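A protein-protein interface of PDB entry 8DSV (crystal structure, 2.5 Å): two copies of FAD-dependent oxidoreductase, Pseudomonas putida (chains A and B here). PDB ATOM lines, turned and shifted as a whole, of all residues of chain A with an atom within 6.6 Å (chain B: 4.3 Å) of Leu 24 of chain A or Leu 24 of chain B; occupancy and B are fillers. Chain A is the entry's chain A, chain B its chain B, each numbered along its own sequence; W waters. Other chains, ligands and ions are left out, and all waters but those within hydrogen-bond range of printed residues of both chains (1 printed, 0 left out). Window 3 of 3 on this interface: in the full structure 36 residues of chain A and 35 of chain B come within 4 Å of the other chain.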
ATOM      1  N   ALA A  19      -3.706  15.885  -6.498  1.00  0.00           N
ATOM      2  CA  ALA A  19      -3.912  16.634  -5.267  1.00  0.00           C
ATOM      3  C   ALA A  19      -3.619  18.108  -5.475  1.00  0.00           C
ATOM      4  O   ALA A  19      -4.331  18.966  -4.946  1.00  0.00           O
ATOM      5  CB  ALA A  19      -3.035  16.064  -4.152  1.00  0.00           C
ATOM      6  N   ARG A  20      -2.590  18.424  -6.262  1.00  0.00           N
ATOM      7  CA  ARG A  20      -2.286  19.823  -6.533  1.00  0.00           C
ATOM      8  C   ARG A  20      -3.442  20.492  -7.267  1.00  0.00           C
ATOM      9  O   ARG A  20      -3.891  21.581  -6.886  1.00  0.00           O
ATOM     10  CB  ARG A  20      -0.988  19.927  -7.334  1.00  0.00           C
ATOM     11  CG  ARG A  20      -0.345  21.309  -7.315  1.00  0.00           C
ATOM     12  CD  ARG A  20      -0.895  22.229  -8.405  1.00  0.00           C
ATOM     13  NE  ARG A  20      -1.055  21.555  -9.689  1.00  0.00           N
ATOM     14  CZ  ARG A  20      -0.055  21.212 -10.492  1.00  0.00           C
ATOM     15  NH1 ARG A  20       1.204  21.486 -10.189  1.00  0.00           N
ATOM     16  NH2 ARG A  20      -0.326  20.583 -11.630  1.00  0.00           N
ATOM     17  N   GLU A  21      -3.953  19.838  -8.312  1.00  0.00           N
ATOM     18  CA  GLU A  21      -5.075  20.405  -9.059  1.00  0.00           C
ATOM     19  C   GLU A  21      -6.282  20.633  -8.150  1.00  0.00           C
ATOM     20  O   GLU A  21      -6.851  21.738  -8.098  1.00  0.00           O
ATOM     21  CB  GLU A  21      -5.443  19.482 -10.220  1.00  0.00           C
ATOM     22  CG  GLU A  21      -4.336  19.301 -11.240  1.00  0.00           C
ATOM     23  CD  GLU A  21      -4.066  20.564 -12.023  1.00  0.00           C
ATOM     24  OE1 GLU A  21      -4.813  20.838 -12.983  1.00  0.00           O
ATOM     25  OE2 GLU A  21      -3.113  21.287 -11.669  1.00  0.00           O
ATOM     26  N   CYS A  22      -6.674  19.599  -7.407  1.00  0.00           N
ATOM     27  CA  CYS A  22      -7.866  19.709  -6.576  1.00  0.00           C
ATOM     28  C   CYS A  22      -7.691  20.770  -5.498  1.00  0.00           C
ATOM     29  O   CYS A  22      -8.601  21.571  -5.257  1.00  0.00           O
ATOM     30  CB  CYS A  22      -8.192  18.351  -5.958  1.00  0.00           C
ATOM     31  SG  CYS A  22      -8.765  17.136  -7.173  1.00  0.00           S
ATOM     32  N   GLY A  23      -6.522  20.814  -4.859  1.00  0.00           N
ATOM     33  CA  GLY A  23      -6.305  21.788  -3.806  1.00  0.00           C
ATOM     34  C   GLY A  23      -6.334  23.210  -4.321  1.00  0.00           C
ATOM     35  O   GLY A  23      -6.948  24.088  -3.711  1.00  0.00           O
ATOM     36  N   LEU A  24      -5.691  23.459  -5.463  1.00  0.00           N
ATOM     37  CA  LEU A  24      -5.717  24.812  -5.991  1.00  0.00           C
ATOM     38  C   LEU A  24      -7.081  25.181  -6.545  1.00  0.00           C
ATOM     39  O   LEU A  24      -7.323  26.366  -6.799  1.00  0.00           O
ATOM     40  CB  LEU A  24      -4.636  24.988  -7.056  1.00  0.00           C
ATOM     41  CG  LEU A  24      -3.190  24.928  -6.546  1.00  0.00           C
ATOM     42  CD1 LEU A  24      -2.232  25.421  -7.619  1.00  0.00           C
ATOM     43  CD2 LEU A  24      -3.009  25.733  -5.271  1.00  0.00           C
ATOM     44  N   GLN A  25      -7.980  24.211  -6.729  1.00  0.00           N
ATOM     45  CA  GLN A  25      -9.366  24.572  -7.014  1.00  0.00           C
ATOM     46  C   GLN A  25     -10.158  24.907  -5.756  1.00  0.00           C
ATOM     47  O   GLN A  25     -11.338  25.257  -5.863  1.00  0.00           O
ATOM     48  CB  GLN A  25     -10.073  23.449  -7.772  1.00  0.00           C
ATOM     49  CG  GLN A  25      -9.630  23.307  -9.219  1.00  0.00           C
ATOM     50  CD  GLN A  25      -9.782  24.591 -10.006  1.00  0.00           C
ATOM     51  OE1 GLN A  25     -10.889  25.103 -10.177  1.00  0.00           O
ATOM     52  NE2 GLN A  25      -8.664  25.122 -10.487  1.00  0.00           N
ATOM     53  N   GLY A  26      -9.557  24.793  -4.574  1.00  0.00           N
ATOM     54  CA  GLY A  26     -10.219  25.158  -3.341  1.00  0.00           C
ATOM     55  C   GLY A  26     -10.934  24.028  -2.635  1.00  0.00           C
ATOM     56  O   GLY A  26     -11.564  24.268  -1.595  1.00  0.00           O
ATOM     57  N   TYR A  27     -10.867  22.811  -3.162  1.00  0.00           N
ATOM     58  CA  TYR A  27     -11.491  21.671  -2.508  1.00  0.00           C
ATOM     59  C   TYR A  27     -10.723  21.281  -1.249  1.00  0.00           C
ATOM     60  O   TYR A  27      -9.497  21.422  -1.170  1.00  0.00           O
ATOM     61  CB  TYR A  27     -11.548  20.479  -3.466  1.00  0.00           C
ATOM     62  CG  TYR A  27     -12.298  20.766  -4.745  1.00  0.00           C
ATOM     63  CD1 TYR A  27     -13.512  21.445  -4.722  1.00  0.00           C
ATOM     64  CD2 TYR A  27     -11.796  20.363  -5.974  1.00  0.00           C
ATOM     65  CE1 TYR A  27     -14.203  21.715  -5.888  1.00  0.00           C
ATOM     66  CE2 TYR A  27     -12.481  20.628  -7.149  1.00  0.00           C
ATOM     67  CZ  TYR A  27     -13.682  21.305  -7.099  1.00  0.00           C
ATOM     68  OH  TYR A  27     -14.369  21.576  -8.258  1.00  0.00           O
ATOM     69  N   THR A  29      -9.000  18.658   0.483  1.00  0.00           N
ATOM     70  CA  THR A  29      -8.355  17.536  -0.182  1.00  0.00           C
ATOM     71  C   THR A  29      -7.520  16.737   0.809  1.00  0.00           C
ATOM     72  O   THR A  29      -6.736  17.310   1.570  1.00  0.00           O
ATOM     73  CB  THR A  29      -7.466  18.035  -1.322  1.00  0.00           C
ATOM     74  OG1 THR A  29      -8.268  18.730  -2.287  1.00  0.00           O
ATOM     75  CG2 THR A  29      -6.752  16.882  -1.985  1.00  0.00           C
ATOM     76  N   ARG A  72       6.810  25.390 -14.123  1.00  0.00           N
ATOM     77  CA  ARG A  72       6.011  26.009 -13.072  1.00  0.00           C
ATOM     78  C   ARG A  72       6.818  26.172 -11.788  1.00  0.00           C
ATOM     79  O   ARG A  72       6.767  27.226 -11.144  1.00  0.00           O
ATOM     80  CB  ARG A  72       4.751  25.173 -12.827  1.00  0.00           C
ATOM     81  CG  ARG A  72       4.024  25.448 -11.516  1.00  0.00           C
ATOM     82  CD  ARG A  72       2.691  24.698 -11.467  1.00  0.00           C
ATOM     83  NE  ARG A  72       1.714  25.290 -12.376  1.00  0.00           N
ATOM     84  CZ  ARG A  72       1.247  24.716 -13.479  1.00  0.00           C
ATOM     85  NH1 ARG A  72       1.568  23.474 -13.812  1.00  0.00           N
ATOM     86  NH2 ARG A  72       0.434  25.407 -14.272  1.00  0.00           N
ATOM     87  N   TYR A  73       7.585  25.151 -11.407  1.00  0.00           N
ATOM     88  CA  TYR A  73       8.312  25.184 -10.144  1.00  0.00           C
ATOM     89  C   TYR A  73       9.792  25.521 -10.312  1.00  0.00           C
ATOM     90  O   TYR A  73      10.544  25.462  -9.334  1.00  0.00           O
ATOM     91  CB  TYR A  73       8.138  23.853  -9.409  1.00  0.00           C
ATOM     92  CG  TYR A  73       6.695  23.593  -9.041  1.00  0.00           C
ATOM     93  CD1 TYR A  73       6.090  24.284  -7.999  1.00  0.00           C
ATOM     94  CD2 TYR A  73       5.927  22.684  -9.757  1.00  0.00           C
ATOM     95  CE1 TYR A  73       4.768  24.065  -7.671  1.00  0.00           C
ATOM     96  CE2 TYR A  73       4.605  22.458  -9.434  1.00  0.00           C
ATOM     97  CZ  TYR A  73       4.029  23.151  -8.392  1.00  0.00           C
ATOM     98  OH  TYR A  73       2.707  22.926  -8.072  1.00  0.00           O
ATOM     99  N   ASP A 218       2.273  23.140  -2.613  1.00  0.00           N
ATOM    100  CA  ASP A 218       1.412  24.050  -3.355  1.00  0.00           C
ATOM    101  C   ASP A 218      -0.055  23.692  -3.166  1.00  0.00           C
ATOM    102  O   ASP A 218      -0.910  24.583  -3.115  1.00  0.00           O
ATOM    103  CB  ASP A 218       1.800  24.005  -4.837  1.00  0.00           C
ATOM    104  CG  ASP A 218       1.197  25.136  -5.648  1.00  0.00           C
ATOM    105  OD1 ASP A 218       0.701  26.114  -5.056  1.00  0.00           O
ATOM    106  OD2 ASP A 218       1.231  25.044  -6.893  1.00  0.00           O
ATOM    107  N   SER A 219      -0.358  22.394  -3.041  1.00  0.00           N
ATOM    108  CA  SER A 219      -1.746  21.939  -3.018  1.00  0.00           C
ATOM    109  C   SER A 219      -2.468  22.331  -1.736  1.00  0.00           C
ATOM    110  O   SER A 219      -3.687  22.534  -1.753  1.00  0.00           O
ATOM    111  CB  SER A 219      -1.796  20.422  -3.194  1.00  0.00           C
ATOM    112  OG  SER A 219      -1.529  19.750  -1.978  1.00  0.00           O
ATOM    113  N   GLY A 220      -1.757  22.422  -0.619  1.00  0.00           N
ATOM    114  CA  GLY A 220      -2.418  22.626   0.650  1.00  0.00           C
ATOM    115  C   GLY A 220      -3.142  21.413   1.192  1.00  0.00           C
ATOM    116  O   GLY A 220      -3.803  21.523   2.231  1.00  0.00           O
ATOM    117  N   ARG B  20      -4.096  33.010 -14.544  1.00  0.00           N
ATOM    118  CA  ARG B  20      -4.589  31.746 -14.006  1.00  0.00           C
ATOM    119  C   ARG B  20      -3.713  31.271 -12.851  1.00  0.00           C
ATOM    120  O   ARG B  20      -4.216  30.895 -11.783  1.00  0.00           O
ATOM    121  CB  ARG B  20      -4.646  30.703 -15.124  1.00  0.00           C
ATOM    122  CG  ARG B  20      -5.528  29.499 -14.826  1.00  0.00           C
ATOM    123  CD  ARG B  20      -4.816  28.447 -13.987  1.00  0.00           C
ATOM    124  NE  ARG B  20      -3.478  28.152 -14.482  1.00  0.00           N
ATOM    125  CZ  ARG B  20      -3.219  27.487 -15.600  1.00  0.00           C
ATOM    126  NH1 ARG B  20      -4.190  27.008 -16.361  1.00  0.00           N
ATOM    127  NH2 ARG B  20      -1.954  27.294 -15.962  1.00  0.00           N
ATOM    128  N   GLU B  21      -2.391  31.300 -13.044  1.00  0.00           N
ATOM    129  CA  GLU B  21      -1.477  30.898 -11.979  1.00  0.00           C
ATOM    130  C   GLU B  21      -1.684  31.751 -10.735  1.00  0.00           C
ATOM    131  O   GLU B  21      -1.809  31.226  -9.623  1.00  0.00           O
ATOM    132  CB  GLU B  21      -0.028  30.997 -12.457  1.00  0.00           C
ATOM    133  CG  GLU B  21       0.352  29.999 -13.547  1.00  0.00           C
ATOM    134  CD  GLU B  21       0.344  28.557 -13.067  1.00  0.00           C
ATOM    135  OE1 GLU B  21       1.349  28.116 -12.463  1.00  0.00           O
ATOM    136  OE2 GLU B  21      -0.664  27.859 -13.306  1.00  0.00           O
ATOM    137  N   CYS B  22      -1.705  33.077 -10.901  1.00  0.00           N
ATOM    138  CA  CYS B  22      -1.846  33.967  -9.751  1.00  0.00           C
ATOM    139  C   CYS B  22      -3.199  33.787  -9.067  1.00  0.00           C
ATOM    140  O   CYS B  22      -3.282  33.769  -7.833  1.00  0.00           O
ATOM    141  CB  CYS B  22      -1.660  35.418 -10.188  1.00  0.00           C
ATOM    142  SG  CYS B  22       0.023  35.815 -10.706  1.00  0.00           S
ATOM    143  N   GLY B  23      -4.271  33.659  -9.850  1.00  0.00           N
ATOM    144  CA  GLY B  23      -5.592  33.518  -9.270  1.00  0.00           C
ATOM    145  C   GLY B  23      -5.745  32.241  -8.470  1.00  0.00           C
ATOM    146  O   GLY B  23      -6.357  32.243  -7.399  1.00  0.00           O
ATOM    147  N   LEU B  24      -5.198  31.130  -8.980  1.00  0.00           N
ATOM    148  CA  LEU B  24      -5.304  29.879  -8.237  1.00  0.00           C
ATOM    149  C   LEU B  24      -4.438  29.853  -6.982  1.00  0.00           C
ATOM    150  O   LEU B  24      -4.629  28.967  -6.143  1.00  0.00           O
ATOM    151  CB  LEU B  24      -4.932  28.699  -9.135  1.00  0.00           C
ATOM    152  CG  LEU B  24      -5.867  28.406 -10.312  1.00  0.00           C
ATOM    153  CD1 LEU B  24      -5.575  27.032 -10.869  1.00  0.00           C
ATOM    154  CD2 LEU B  24      -7.324  28.514  -9.910  1.00  0.00           C
ATOM    155  N   GLN B  25      -3.501  30.788  -6.827  1.00  0.00           N
ATOM    156  CA  GLN B  25      -2.784  30.945  -5.566  1.00  0.00           C
ATOM    157  C   GLN B  25      -3.528  31.815  -4.560  1.00  0.00           C
ATOM    158  O   GLN B  25      -3.059  31.965  -3.426  1.00  0.00           O
ATOM    159  CB  GLN B  25      -1.394  31.536  -5.815  1.00  0.00           C
ATOM    160  CG  GLN B  25      -0.484  30.640  -6.626  1.00  0.00           C
ATOM    161  CD  GLN B  25      -0.068  29.396  -5.868  1.00  0.00           C
ATOM    162  OE1 GLN B  25       0.270  29.459  -4.689  1.00  0.00           O
ATOM    163  NE2 GLN B  25      -0.091  28.254  -6.546  1.00  0.00           N
ATOM    164  N   GLY B  26      -4.666  32.392  -4.935  1.00  0.00           N
ATOM    165  CA  GLY B  26      -5.454  33.179  -4.011  1.00  0.00           C
ATOM    166  C   GLY B  26      -5.168  34.665  -4.015  1.00  0.00           C
ATOM    167  O   GLY B  26      -5.760  35.394  -3.210  1.00  0.00           O
ATOM    168  N   ASP B 218     -11.148  29.905 -14.998  1.00  0.00           N
ATOM    169  CA  ASP B 218     -10.518  29.184 -13.900  1.00  0.00           C
ATOM    170  C   ASP B 218      -9.840  30.139 -12.927  1.00  0.00           C
ATOM    171  O   ASP B 218      -9.856  29.904 -11.714  1.00  0.00           O
ATOM    172  CB  ASP B 218      -9.504  28.181 -14.462  1.00  0.00           C
ATOM    173  CG  ASP B 218      -9.143  27.080 -13.474  1.00  0.00           C
ATOM    174  OD1 ASP B 218      -9.736  27.031 -12.377  1.00  0.00           O
ATOM    175  OD2 ASP B 218      -8.255  26.261 -13.799  1.00  0.00           O
HETATM  176  O   HOH W   1     -11.348  27.930 -10.111  1.00  0.00           O
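OD1 of Asp 218 of chain B is in hydrogen-bond range of NE2 of Gln 25 of chain A, 2.9 Å away. The side-chain carboxylate of Glu 21 of chain B lies within salt-bridge range of the guanidinium group of Arg 72 of chain A, 2.9 Å away. NE2 of Gln 25 of chain B is in hydrogen-bond range of OD1 of Asp 218 of chain A, at 2.7 Å. The guanidinium group of Arg 72 of chain A sits close to the guanidinium group of Arg 20 of chain B (3.5 Å).
Of chain B, only Leu 24 and Gln 25 come within 4 Å of Leu 24 of chain A. Leu 24 of chain B touches two residues of chain A. Of the printed residues of chain B, Asp 218 of chain A touches Gln 25 (2.7 Å). Of the printed residues of chain A, Gln 25 of chain B touches Leu 24 (3.7 Å) and Asp 218 (2.7 Å). Printed residues of chain A within 4 Å of Asp 218 of chain B: Gln 25. Printed residues of chain B within 4 Å of Gln 25 of chain A: Leu 24 (3.7 Å) and Asp 218 (2.9 Å). Of the printed residues of chain A, Arg 20 of chain B touches Arg 72.
Water W1 bridges OE1 of Gln 25 of chain A and OD1 of Asp 218 of chain B.
Leu 24 of chain A touches its own counterpart, Leu 24 of chain B. Leu 24 of chain A touches Gln 25 of chain B, and with the chains exchanged Gln 25 of chain A touches Leu 24 of chain B. Gln 25 of chain A touches Asp 218 of chain B, and with the chains exchanged Asp 218 of chain A touches Gln 25 of chain B.
Leu 24 of chain A touches Leu 24 of chain B. Gln 25 of chain B touches Leu 24 of chain A (NE2 to CD1, 3.7 Å). NE2 of Gln 25 of chain A touches CD1 of Leu 24 of chain B, at 3.7 Å.
Of the 8 printed residues of chain B, 5 touch a printed residue of chain A. Among the printed residues, 7 pairs touch across the chains. Among the printed residues, Asp or Glu carboxylates within 4 Å of a Lys or Arg side-chain nitrogen of the other chain: Arg 72 of chain A with Glu 21 of chain B (2.9 Å).
OD2 of Asp 218 of chain A is in hydrogen-bond range of OH of Tyr 73 of chain A (2.8 Å). NH2 of Arg 20 of chain B lies within salt-bridge range of OE2 of Glu 21 of chain B (3.0 Å).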
